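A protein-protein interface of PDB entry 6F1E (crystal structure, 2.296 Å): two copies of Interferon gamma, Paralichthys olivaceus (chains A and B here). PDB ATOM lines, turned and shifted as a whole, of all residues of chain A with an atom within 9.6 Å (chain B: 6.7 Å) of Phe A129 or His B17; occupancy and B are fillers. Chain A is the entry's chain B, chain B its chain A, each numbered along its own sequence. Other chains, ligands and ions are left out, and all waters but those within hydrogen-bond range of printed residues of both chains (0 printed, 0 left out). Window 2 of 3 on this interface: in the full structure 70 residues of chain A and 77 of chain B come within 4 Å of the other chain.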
ATOM      1  N   LYS A 125      10.898  35.260 -12.793  1.00  0.00           N
ATOM      2  CA  LYS A 125      10.587  36.164 -11.662  1.00  0.00           C
ATOM      3  C   LYS A 125      10.167  35.401 -10.363  1.00  0.00           C
ATOM      4  O   LYS A 125       8.976  35.173 -10.070  1.00  0.00           O
ATOM      5  CB  LYS A 125       9.560  37.234 -12.099  1.00  0.00           C
ATOM      6  CG  LYS A 125      10.190  38.437 -12.824  1.00  0.00           C
ATOM      7  CD  LYS A 125       9.296  39.116 -13.882  1.00  0.00           C
ATOM      8  CE  LYS A 125       9.815  38.896 -15.319  1.00  0.00           C
ATOM      9  NZ  LYS A 125       8.964  39.425 -16.437  1.00  0.00           N
ATOM     10  N   MET A 126      11.180  35.021  -9.591  1.00  0.00           N
ATOM     11  CA  MET A 126      11.030  34.319  -8.290  1.00  0.00           C
ATOM     12  C   MET A 126       9.921  34.832  -7.335  1.00  0.00           C
ATOM     13  O   MET A 126       9.322  34.035  -6.627  1.00  0.00           O
ATOM     14  CB  MET A 126      12.356  34.373  -7.491  1.00  0.00           C
ATOM     15  CG  MET A 126      13.609  33.769  -8.122  1.00  0.00           C
ATOM     16  SD  MET A 126      13.407  32.084  -8.717  1.00  0.00           S
ATOM     17  CE  MET A 126      14.944  31.885  -9.639  1.00  0.00           C
ATOM     18  N   ASN A 127       9.686  36.143  -7.295  1.00  0.00           N
ATOM     19  CA  ASN A 127       8.761  36.780  -6.340  1.00  0.00           C
ATOM     20  C   ASN A 127       7.308  36.872  -6.808  1.00  0.00           C
ATOM     21  O   ASN A 127       6.403  37.164  -6.008  1.00  0.00           O
ATOM     22  CB  ASN A 127       9.243  38.195  -6.024  1.00  0.00           C
ATOM     23  CG  ASN A 127      10.597  38.218  -5.332  1.00  0.00           C
ATOM     24  OD1 ASN A 127      11.279  37.185  -5.201  1.00  0.00           O
ATOM     25  ND2 ASN A 127      10.995  39.408  -4.875  1.00  0.00           N
ATOM     26  N   ASN A 128       7.087  36.626  -8.095  1.00  0.00           N
ATOM     27  CA  ASN A 128       5.777  36.785  -8.715  1.00  0.00           C
ATOM     28  C   ASN A 128       4.903  35.612  -8.347  1.00  0.00           C
ATOM     29  O   ASN A 128       5.277  34.469  -8.621  1.00  0.00           O
ATOM     30  CB  ASN A 128       5.949  36.849 -10.243  1.00  0.00           C
ATOM     31  CG  ASN A 128       4.691  37.280 -10.966  1.00  0.00           C
ATOM     32  OD1 ASN A 128       3.725  36.514 -11.086  1.00  0.00           O
ATOM     33  ND2 ASN A 128       4.710  38.502 -11.482  1.00  0.00           N
ATOM     34  N   PHE A 129       3.732  35.903  -7.773  1.00  0.00           N
ATOM     35  CA  PHE A 129       2.760  34.872  -7.357  1.00  0.00           C
ATOM     36  C   PHE A 129       2.264  33.964  -8.518  1.00  0.00           C
ATOM     37  O   PHE A 129       2.145  32.737  -8.341  1.00  0.00           O
ATOM     38  CB  PHE A 129       1.563  35.531  -6.651  1.00  0.00           C
ATOM     39  CG  PHE A 129       0.626  34.549  -5.964  1.00  0.00           C
ATOM     40  CD1 PHE A 129       0.837  34.162  -4.638  1.00  0.00           C
ATOM     41  CD2 PHE A 129      -0.484  34.015  -6.635  1.00  0.00           C
ATOM     42  CE1 PHE A 129      -0.027  33.270  -4.000  1.00  0.00           C
ATOM     43  CE2 PHE A 129      -1.349  33.107  -5.997  1.00  0.00           C
ATOM     44  CZ  PHE A 129      -1.121  32.742  -4.681  1.00  0.00           C
ATOM     45  N   ILE A 130       1.993  34.542  -9.696  1.00  0.00           N
ATOM     46  CA  ILE A 130       1.475  33.747 -10.846  1.00  0.00           C
ATOM     47  C   ILE A 130       2.514  32.701 -11.320  1.00  0.00           C
ATOM     48  O   ILE A 130       2.198  31.511 -11.533  1.00  0.00           O
ATOM     49  CB  ILE A 130       1.112  34.628 -12.080  1.00  0.00           C
ATOM     50  CG1 ILE A 130       0.054  35.719 -11.753  1.00  0.00           C
ATOM     51  CG2 ILE A 130       0.636  33.744 -13.244  1.00  0.00           C
ATOM     52  CD1 ILE A 130      -1.257  35.236 -11.190  1.00  0.00           C
ATOM     53  N   ILE A 131       3.741  33.186 -11.481  1.00  0.00           N
ATOM     54  CA  ILE A 131       4.899  32.365 -11.807  1.00  0.00           C
ATOM     55  C   ILE A 131       5.149  31.254 -10.781  1.00  0.00           C
ATOM     56  O   ILE A 131       5.397  30.081 -11.166  1.00  0.00           O
ATOM     57  CB  ILE A 131       6.148  33.252 -11.933  1.00  0.00           C
ATOM     58  CG1 ILE A 131       5.867  34.298 -13.054  1.00  0.00           C
ATOM     59  CG2 ILE A 131       7.406  32.397 -12.139  1.00  0.00           C
ATOM     60  CD1 ILE A 131       7.049  34.721 -13.895  1.00  0.00           C
ATOM     61  N   GLN A 132       5.071  31.617  -9.496  1.00  0.00           N
ATOM     62  CA  GLN A 132       5.177  30.622  -8.427  1.00  0.00           C
ATOM     63  C   GLN A 132       4.168  29.508  -8.608  1.00  0.00           C
ATOM     64  O   GLN A 132       4.495  28.324  -8.465  1.00  0.00           O
ATOM     65  CB  GLN A 132       4.995  31.252  -7.041  1.00  0.00           C
ATOM     66  CG  GLN A 132       6.246  31.970  -6.559  1.00  0.00           C
ATOM     67  CD  GLN A 132       5.994  32.871  -5.368  1.00  0.00           C
ATOM     68  OE1 GLN A 132       4.906  32.876  -4.771  1.00  0.00           O
ATOM     69  NE2 GLN A 132       7.011  33.634  -5.004  1.00  0.00           N
ATOM     70  N   SER A 133       2.951  29.898  -8.940  1.00  0.00           N
ATOM     71  CA  SER A 133       1.881  28.940  -9.057  1.00  0.00           C
ATOM     72  C   SER A 133       1.937  28.213 -10.352  1.00  0.00           C
ATOM     73  O   SER A 133       1.458  27.082 -10.418  1.00  0.00           O
ATOM     74  CB  SER A 133       0.521  29.623  -8.967  1.00  0.00           C
ATOM     75  OG  SER A 133      -0.506  28.648  -9.149  1.00  0.00           O
ATOM     76  N   LYS A 134       2.449  28.868 -11.401  1.00  0.00           N
ATOM     77  CA  LYS A 134       2.645  28.179 -12.704  1.00  0.00           C
ATOM     78  C   LYS A 134       3.755  27.120 -12.597  1.00  0.00           C
ATOM     79  O   LYS A 134       3.541  25.955 -12.935  1.00  0.00           O
ATOM     80  CB  LYS A 134       2.911  29.172 -13.850  1.00  0.00           C
ATOM     81  CG  LYS A 134       1.650  29.903 -14.317  1.00  0.00           C
ATOM     82  CD  LYS A 134       1.954  31.045 -15.275  1.00  0.00           C
ATOM     83  CE  LYS A 134       2.212  30.517 -16.674  1.00  0.00           C
ATOM     84  NZ  LYS A 134       2.161  31.645 -17.652  1.00  0.00           N
ATOM     85  N   ALA A 135       4.914  27.535 -12.080  1.00  0.00           N
ATOM     86  CA  ALA A 135       6.002  26.618 -11.732  1.00  0.00           C
ATOM     87  C   ALA A 135       5.529  25.417 -10.902  1.00  0.00           C
ATOM     88  O   ALA A 135       5.823  24.236 -11.229  1.00  0.00           O
ATOM     89  CB  ALA A 135       7.065  27.371 -10.962  1.00  0.00           C
ATOM     90  N   LEU A 136       4.770  25.724  -9.848  1.00  0.00           N
ATOM     91  CA  LEU A 136       4.194  24.684  -8.974  1.00  0.00           C
ATOM     92  C   LEU A 136       3.429  23.646  -9.771  1.00  0.00           C
ATOM     93  O   LEU A 136       3.688  22.437  -9.633  1.00  0.00           O
ATOM     94  CB  LEU A 136       3.278  25.301  -7.931  1.00  0.00           C
ATOM     95  CG  LEU A 136       3.245  24.775  -6.495  1.00  0.00           C
ATOM     96  CD1 LEU A 136       4.633  24.418  -5.988  1.00  0.00           C
ATOM     97  CD2 LEU A 136       2.602  25.836  -5.589  1.00  0.00           C
ATOM     98  N   TRP A 137       2.526  24.099 -10.646  1.00  0.00           N
ATOM     99  CA  TRP A 137       1.802  23.164 -11.525  1.00  0.00           C
ATOM    100  C   TRP A 137       2.733  22.374 -12.487  1.00  0.00           C
ATOM    101  O   TRP A 137       2.444  21.247 -12.834  1.00  0.00           O
ATOM    102  CB  TRP A 137       0.796  23.950 -12.319  1.00  0.00           C
ATOM    103  CG  TRP A 137      -0.134  23.173 -13.182  1.00  0.00           C
ATOM    104  CD1 TRP A 137       0.147  22.492 -14.350  1.00  0.00           C
ATOM    105  CD2 TRP A 137      -1.543  23.066 -12.986  1.00  0.00           C
ATOM    106  NE1 TRP A 137      -1.013  21.935 -14.859  1.00  0.00           N
ATOM    107  CE2 TRP A 137      -2.059  22.283 -14.043  1.00  0.00           C
ATOM    108  CE3 TRP A 137      -2.418  23.543 -11.994  1.00  0.00           C
ATOM    109  CZ2 TRP A 137      -3.413  21.974 -14.144  1.00  0.00           C
ATOM    110  CZ3 TRP A 137      -3.772  23.238 -12.091  1.00  0.00           C
ATOM    111  CH2 TRP A 137      -4.258  22.455 -13.160  1.00  0.00           C
ATOM    112  N   GLN B  12      -0.857  19.106  -5.196  1.00  0.00           N
ATOM    113  CA  GLN B  12      -2.274  19.485  -5.216  1.00  0.00           C
ATOM    114  C   GLN B  12      -2.662  20.324  -3.992  1.00  0.00           C
ATOM    115  O   GLN B  12      -3.216  21.400  -4.165  1.00  0.00           O
ATOM    116  CB  GLN B  12      -3.179  18.262  -5.348  1.00  0.00           C
ATOM    117  CG  GLN B  12      -2.921  17.370  -6.574  1.00  0.00           C
ATOM    118  CD  GLN B  12      -2.617  18.152  -7.844  1.00  0.00           C
ATOM    119  OE1 GLN B  12      -1.517  18.024  -8.408  1.00  0.00           O
ATOM    120  NE2 GLN B  12      -3.581  18.986  -8.294  1.00  0.00           N
ATOM    121  N   ASN B  13      -2.306  19.887  -2.780  1.00  0.00           N
ATOM    122  CA  ASN B  13      -2.618  20.665  -1.565  1.00  0.00           C
ATOM    123  C   ASN B  13      -2.021  22.042  -1.695  1.00  0.00           C
ATOM    124  O   ASN B  13      -2.649  23.035  -1.351  1.00  0.00           O
ATOM    125  CB  ASN B  13      -2.080  20.046  -0.254  1.00  0.00           C
ATOM    126  CG  ASN B  13      -2.571  18.621  -0.001  1.00  0.00           C
ATOM    127  OD1 ASN B  13      -3.213  17.981  -0.848  1.00  0.00           O
ATOM    128  ND2 ASN B  13      -2.227  18.099   1.176  1.00  0.00           N
ATOM    129  N   LEU B  14      -0.795  22.116  -2.183  1.00  0.00           N
ATOM    130  CA  LEU B  14      -0.152  23.429  -2.365  1.00  0.00           C
ATOM    131  C   LEU B  14      -0.903  24.372  -3.309  1.00  0.00           C
ATOM    132  O   LEU B  14      -0.974  25.602  -3.076  1.00  0.00           O
ATOM    133  CB  LEU B  14       1.279  23.257  -2.825  1.00  0.00           C
ATOM    134  CG  LEU B  14       2.149  22.900  -1.631  1.00  0.00           C
ATOM    135  CD1 LEU B  14       3.347  22.122  -2.148  1.00  0.00           C
ATOM    136  CD2 LEU B  14       2.565  24.151  -0.853  1.00  0.00           C
ATOM    137  N   LEU B  15      -1.461  23.789  -4.363  1.00  0.00           N
ATOM    138  CA  LEU B  15      -2.163  24.575  -5.365  1.00  0.00           C
ATOM    139  C   LEU B  15      -3.427  25.239  -4.809  1.00  0.00           C
ATOM    140  O   LEU B  15      -3.866  26.264  -5.331  1.00  0.00           O
ATOM    141  CB  LEU B  15      -2.447  23.717  -6.600  1.00  0.00           C
ATOM    142  CG  LEU B  15      -1.184  23.431  -7.434  1.00  0.00           C
ATOM    143  CD1 LEU B  15      -1.393  22.230  -8.355  1.00  0.00           C
ATOM    144  CD2 LEU B  15      -0.744  24.680  -8.198  1.00  0.00           C
ATOM    145  N   GLN B  16      -3.986  24.685  -3.735  1.00  0.00           N
ATOM    146  CA  GLN B  16      -5.047  25.382  -2.995  1.00  0.00           C
ATOM    147  C   GLN B  16      -4.626  26.790  -2.507  1.00  0.00           C
ATOM    148  O   GLN B  16      -5.341  27.741  -2.760  1.00  0.00           O
ATOM    149  CB  GLN B  16      -5.589  24.526  -1.824  1.00  0.00           C
ATOM    150  CG  GLN B  16      -6.870  23.746  -2.135  1.00  0.00           C
ATOM    151  CD  GLN B  16      -6.671  22.595  -3.104  1.00  0.00           C
ATOM    152  OE1 GLN B  16      -6.376  21.477  -2.686  1.00  0.00           O
ATOM    153  NE2 GLN B  16      -6.860  22.855  -4.402  1.00  0.00           N
ATOM    154  N   HIS B  17      -3.480  26.929  -1.841  1.00  0.00           N
ATOM    155  CA  HIS B  17      -3.015  28.253  -1.386  1.00  0.00           C
ATOM    156  C   HIS B  17      -2.542  29.073  -2.573  1.00  0.00           C
ATOM    157  O   HIS B  17      -2.627  30.297  -2.536  1.00  0.00           O
ATOM    158  CB  HIS B  17      -1.873  28.118  -0.350  1.00  0.00           C
ATOM    159  CG  HIS B  17      -1.255  29.426   0.096  1.00  0.00           C
ATOM    160  ND1 HIS B  17      -1.636  30.078   1.249  1.00  0.00           N
ATOM    161  CD2 HIS B  17      -0.248  30.170  -0.431  1.00  0.00           C
ATOM    162  CE1 HIS B  17      -0.915  31.180   1.395  1.00  0.00           C
ATOM    163  NE2 HIS B  17      -0.060  31.257   0.391  1.00  0.00           N
ATOM    164  N   TYR B  18      -1.997  28.403  -3.597  1.00  0.00           N
ATOM    165  CA  TYR B  18      -1.344  29.080  -4.735  1.00  0.00           C
ATOM    166  C   TYR B  18      -2.282  28.992  -5.923  1.00  0.00           C
ATOM    167  O   TYR B  18      -2.059  28.228  -6.868  1.00  0.00           O
ATOM    168  CB  TYR B  18       0.018  28.454  -5.013  1.00  0.00           C
ATOM    169  CG  TYR B  18       1.055  28.834  -3.990  1.00  0.00           C
ATOM    170  CD1 TYR B  18       1.557  30.135  -3.955  1.00  0.00           C
ATOM    171  CD2 TYR B  18       1.519  27.922  -3.029  1.00  0.00           C
ATOM    172  CE1 TYR B  18       2.508  30.520  -3.018  1.00  0.00           C
ATOM    173  CE2 TYR B  18       2.475  28.311  -2.080  1.00  0.00           C
ATOM    174  CZ  TYR B  18       2.965  29.616  -2.087  1.00  0.00           C
ATOM    175  OH  TYR B  18       3.906  30.063  -1.194  1.00  0.00           O
ATOM    176  N   ASN B  19      -3.348  29.780  -5.828  1.00  0.00           N
ATOM    177  CA  ASN B  19      -4.552  29.617  -6.634  1.00  0.00           C
ATOM    178  C   ASN B  19      -4.566  30.708  -7.646  1.00  0.00           C
ATOM    179  O   ASN B  19      -4.396  31.874  -7.282  1.00  0.00           O
ATOM    180  CB  ASN B  19      -5.798  29.768  -5.769  1.00  0.00           C
ATOM    181  CG  ASN B  19      -6.973  29.028  -6.342  1.00  0.00           C
ATOM    182  OD1 ASN B  19      -7.385  29.273  -7.479  1.00  0.00           O
ATOM    183  ND2 ASN B  19      -7.506  28.086  -5.567  1.00  0.00           N
ATOM    184  N   ILE B  20      -4.755  30.355  -8.913  1.00  0.00           N
ATOM    185  CA  ILE B  20      -4.843  31.381  -9.945  1.00  0.00           C
ATOM    186  C   ILE B  20      -5.867  30.995 -10.973  1.00  0.00           C
ATOM    187  O   ILE B  20      -6.298  29.828 -11.031  1.00  0.00           O
ATOM    188  CB  ILE B  20      -3.482  31.661 -10.616  1.00  0.00           C
ATOM    189  CG1 ILE B  20      -2.866  30.382 -11.183  1.00  0.00           C
ATOM    190  CG2 ILE B  20      -2.520  32.326  -9.629  1.00  0.00           C
ATOM    191  CD1 ILE B  20      -1.856  30.671 -12.259  1.00  0.00           C
ATOM    192  N   GLN B  65       8.409  34.408   1.542  1.00  0.00           N
ATOM    193  CA  GLN B  65       7.143  35.167   1.407  1.00  0.00           C
ATOM    194  C   GLN B  65       5.967  34.607   2.217  1.00  0.00           C
ATOM    195  O   GLN B  65       4.858  35.137   2.153  1.00  0.00           O
ATOM    196  CB  GLN B  65       6.750  35.315  -0.078  1.00  0.00           C
ATOM    197  CG  GLN B  65       7.581  36.381  -0.784  1.00  0.00           C
ATOM    198  CD  GLN B  65       7.798  36.128  -2.270  1.00  0.00           C
ATOM    199  OE1 GLN B  65       6.849  36.062  -3.057  1.00  0.00           O
ATOM    200  NE2 GLN B  65       9.067  36.012  -2.661  1.00  0.00           N
ATOM    201  N   LEU B  66       6.204  33.533   2.961  1.00  0.00           N
ATOM    202  CA  LEU B  66       5.275  33.075   4.000  1.00  0.00           C
ATOM    203  C   LEU B  66       5.404  33.968   5.276  1.00  0.00           C
ATOM    204  O   LEU B  66       6.532  34.312   5.693  1.00  0.00           O
ATOM    205  CB  LEU B  66       5.558  31.597   4.322  1.00  0.00           C
ATOM    206  CG  LEU B  66       4.432  30.565   4.268  1.00  0.00           C
ATOM    207  CD1 LEU B  66       3.688  30.531   2.932  1.00  0.00           C
ATOM    208  CD2 LEU B  66       5.012  29.183   4.574  1.00  0.00           C
ATOM    209  N   PRO B  67       4.258  34.365   5.886  1.00  0.00           N
ATOM    210  CA  PRO B  67       4.322  35.020   7.213  1.00  0.00           C
ATOM    211  C   PRO B  67       4.562  34.035   8.398  1.00  0.00           C
ATOM    212  O   PRO B  67       4.542  32.801   8.190  1.00  0.00           O
ATOM    213  CB  PRO B  67       2.949  35.709   7.322  1.00  0.00           C
ATOM    214  CG  PRO B  67       2.037  34.891   6.462  1.00  0.00           C
ATOM    215  CD  PRO B  67       2.881  34.365   5.339  1.00  0.00           C
ATOM    216  N   VAL B  89       1.109  24.521   4.742  1.00  0.00           N
ATOM    217  CA  VAL B  89       1.741  25.054   3.538  1.00  0.00           C
ATOM    218  C   VAL B  89       3.259  24.934   3.686  1.00  0.00           C
ATOM    219  O   VAL B  89       3.922  24.334   2.823  1.00  0.00           O
ATOM    220  CB  VAL B  89       1.241  26.499   3.260  1.00  0.00           C
ATOM    221  CG1 VAL B  89       2.242  27.339   2.480  1.00  0.00           C
ATOM    222  CG2 VAL B  89      -0.097  26.425   2.539  1.00  0.00           C
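O of Tyr B18 lies within hydrogen-bond range of OG of Ser A133, 2.8 Å away. The side-chain amide oxygen of Gln B65 sits close to the backbone carbonyl oxygen of Asn A127 (3.2 Å). The side-chain amide oxygen (OE1) of Gln B65 sits at hydrogen-bond distance from the side-chain amide nitrogen (NE2) of Gln A132 (3.1 Å).
O of Met A126 lies within hydrogen-bond range of NE2 of Gln A132. OD1 of Asn A128 is in hydrogen-bond range of N of Ile A130 (3.0 Å).
Phe A129 touches His B17. Phe A129 touches Tyr B18 (CE1 to CD1, 3.5 Å). O of Asn B19 touches CE2 of Phe A129, 3.5 Å away. Ile B20 touches Phe A129 (CG2 to CE2, 3.9 Å). Ile A130 touches Ile B20 (CD1 to CG2, 3.5 Å). Tyr B18 touches Gln A132. Leu B15 touches Ser A133. Ile B20 touches Ser A133. Leu A136 touches Tyr B18.
Of chain B, only His B17, Tyr B18, Asn B19 and Ile B20 come within 4 Å of Phe A129. His B17 touches just one residue of chain A: Phe A129 (3.6 Å). Tyr B18 touches just these residues of chain A: Phe A129, Gln A132, Ser A133 and Leu A136. Printed residues of chain A within 4 Å of Gln B65: Asn A127 and Gln A132. Of the printed residues of chain A, Asn B19 touches Phe A129 (3.5 Å). Of the printed residues of chain B, Asn A127 touches Gln B65 (3.2 Å). The nearest printed residue of chain B that does not touch Asn A127 is Tyr B18 (8.3 Å).
Printed residues of chain B that touch a printed residue of chain A: Leu B15, His B17, Tyr B18, Asn B19, Ile B20 and Gln B65. Hydrophobic or aromatic side chains of chain B that line the printed part of chain A: Leu B15, Tyr B18 and Ile B20. Printed residues of chain A that touch a printed residue of chain B: Asn A127, Phe A129, Ile A130, Gln A132, Ser A133 and Leu A136. Among the printed residues, no Asp or Glu carboxylate lies within 4 Å of a Lys or Arg side-chain nitrogen of the other chain.
No position is printed for both chains. Of the 12 pairs that touch across the chains among the printed residues, none has its exchanged pair printed and touching as well.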
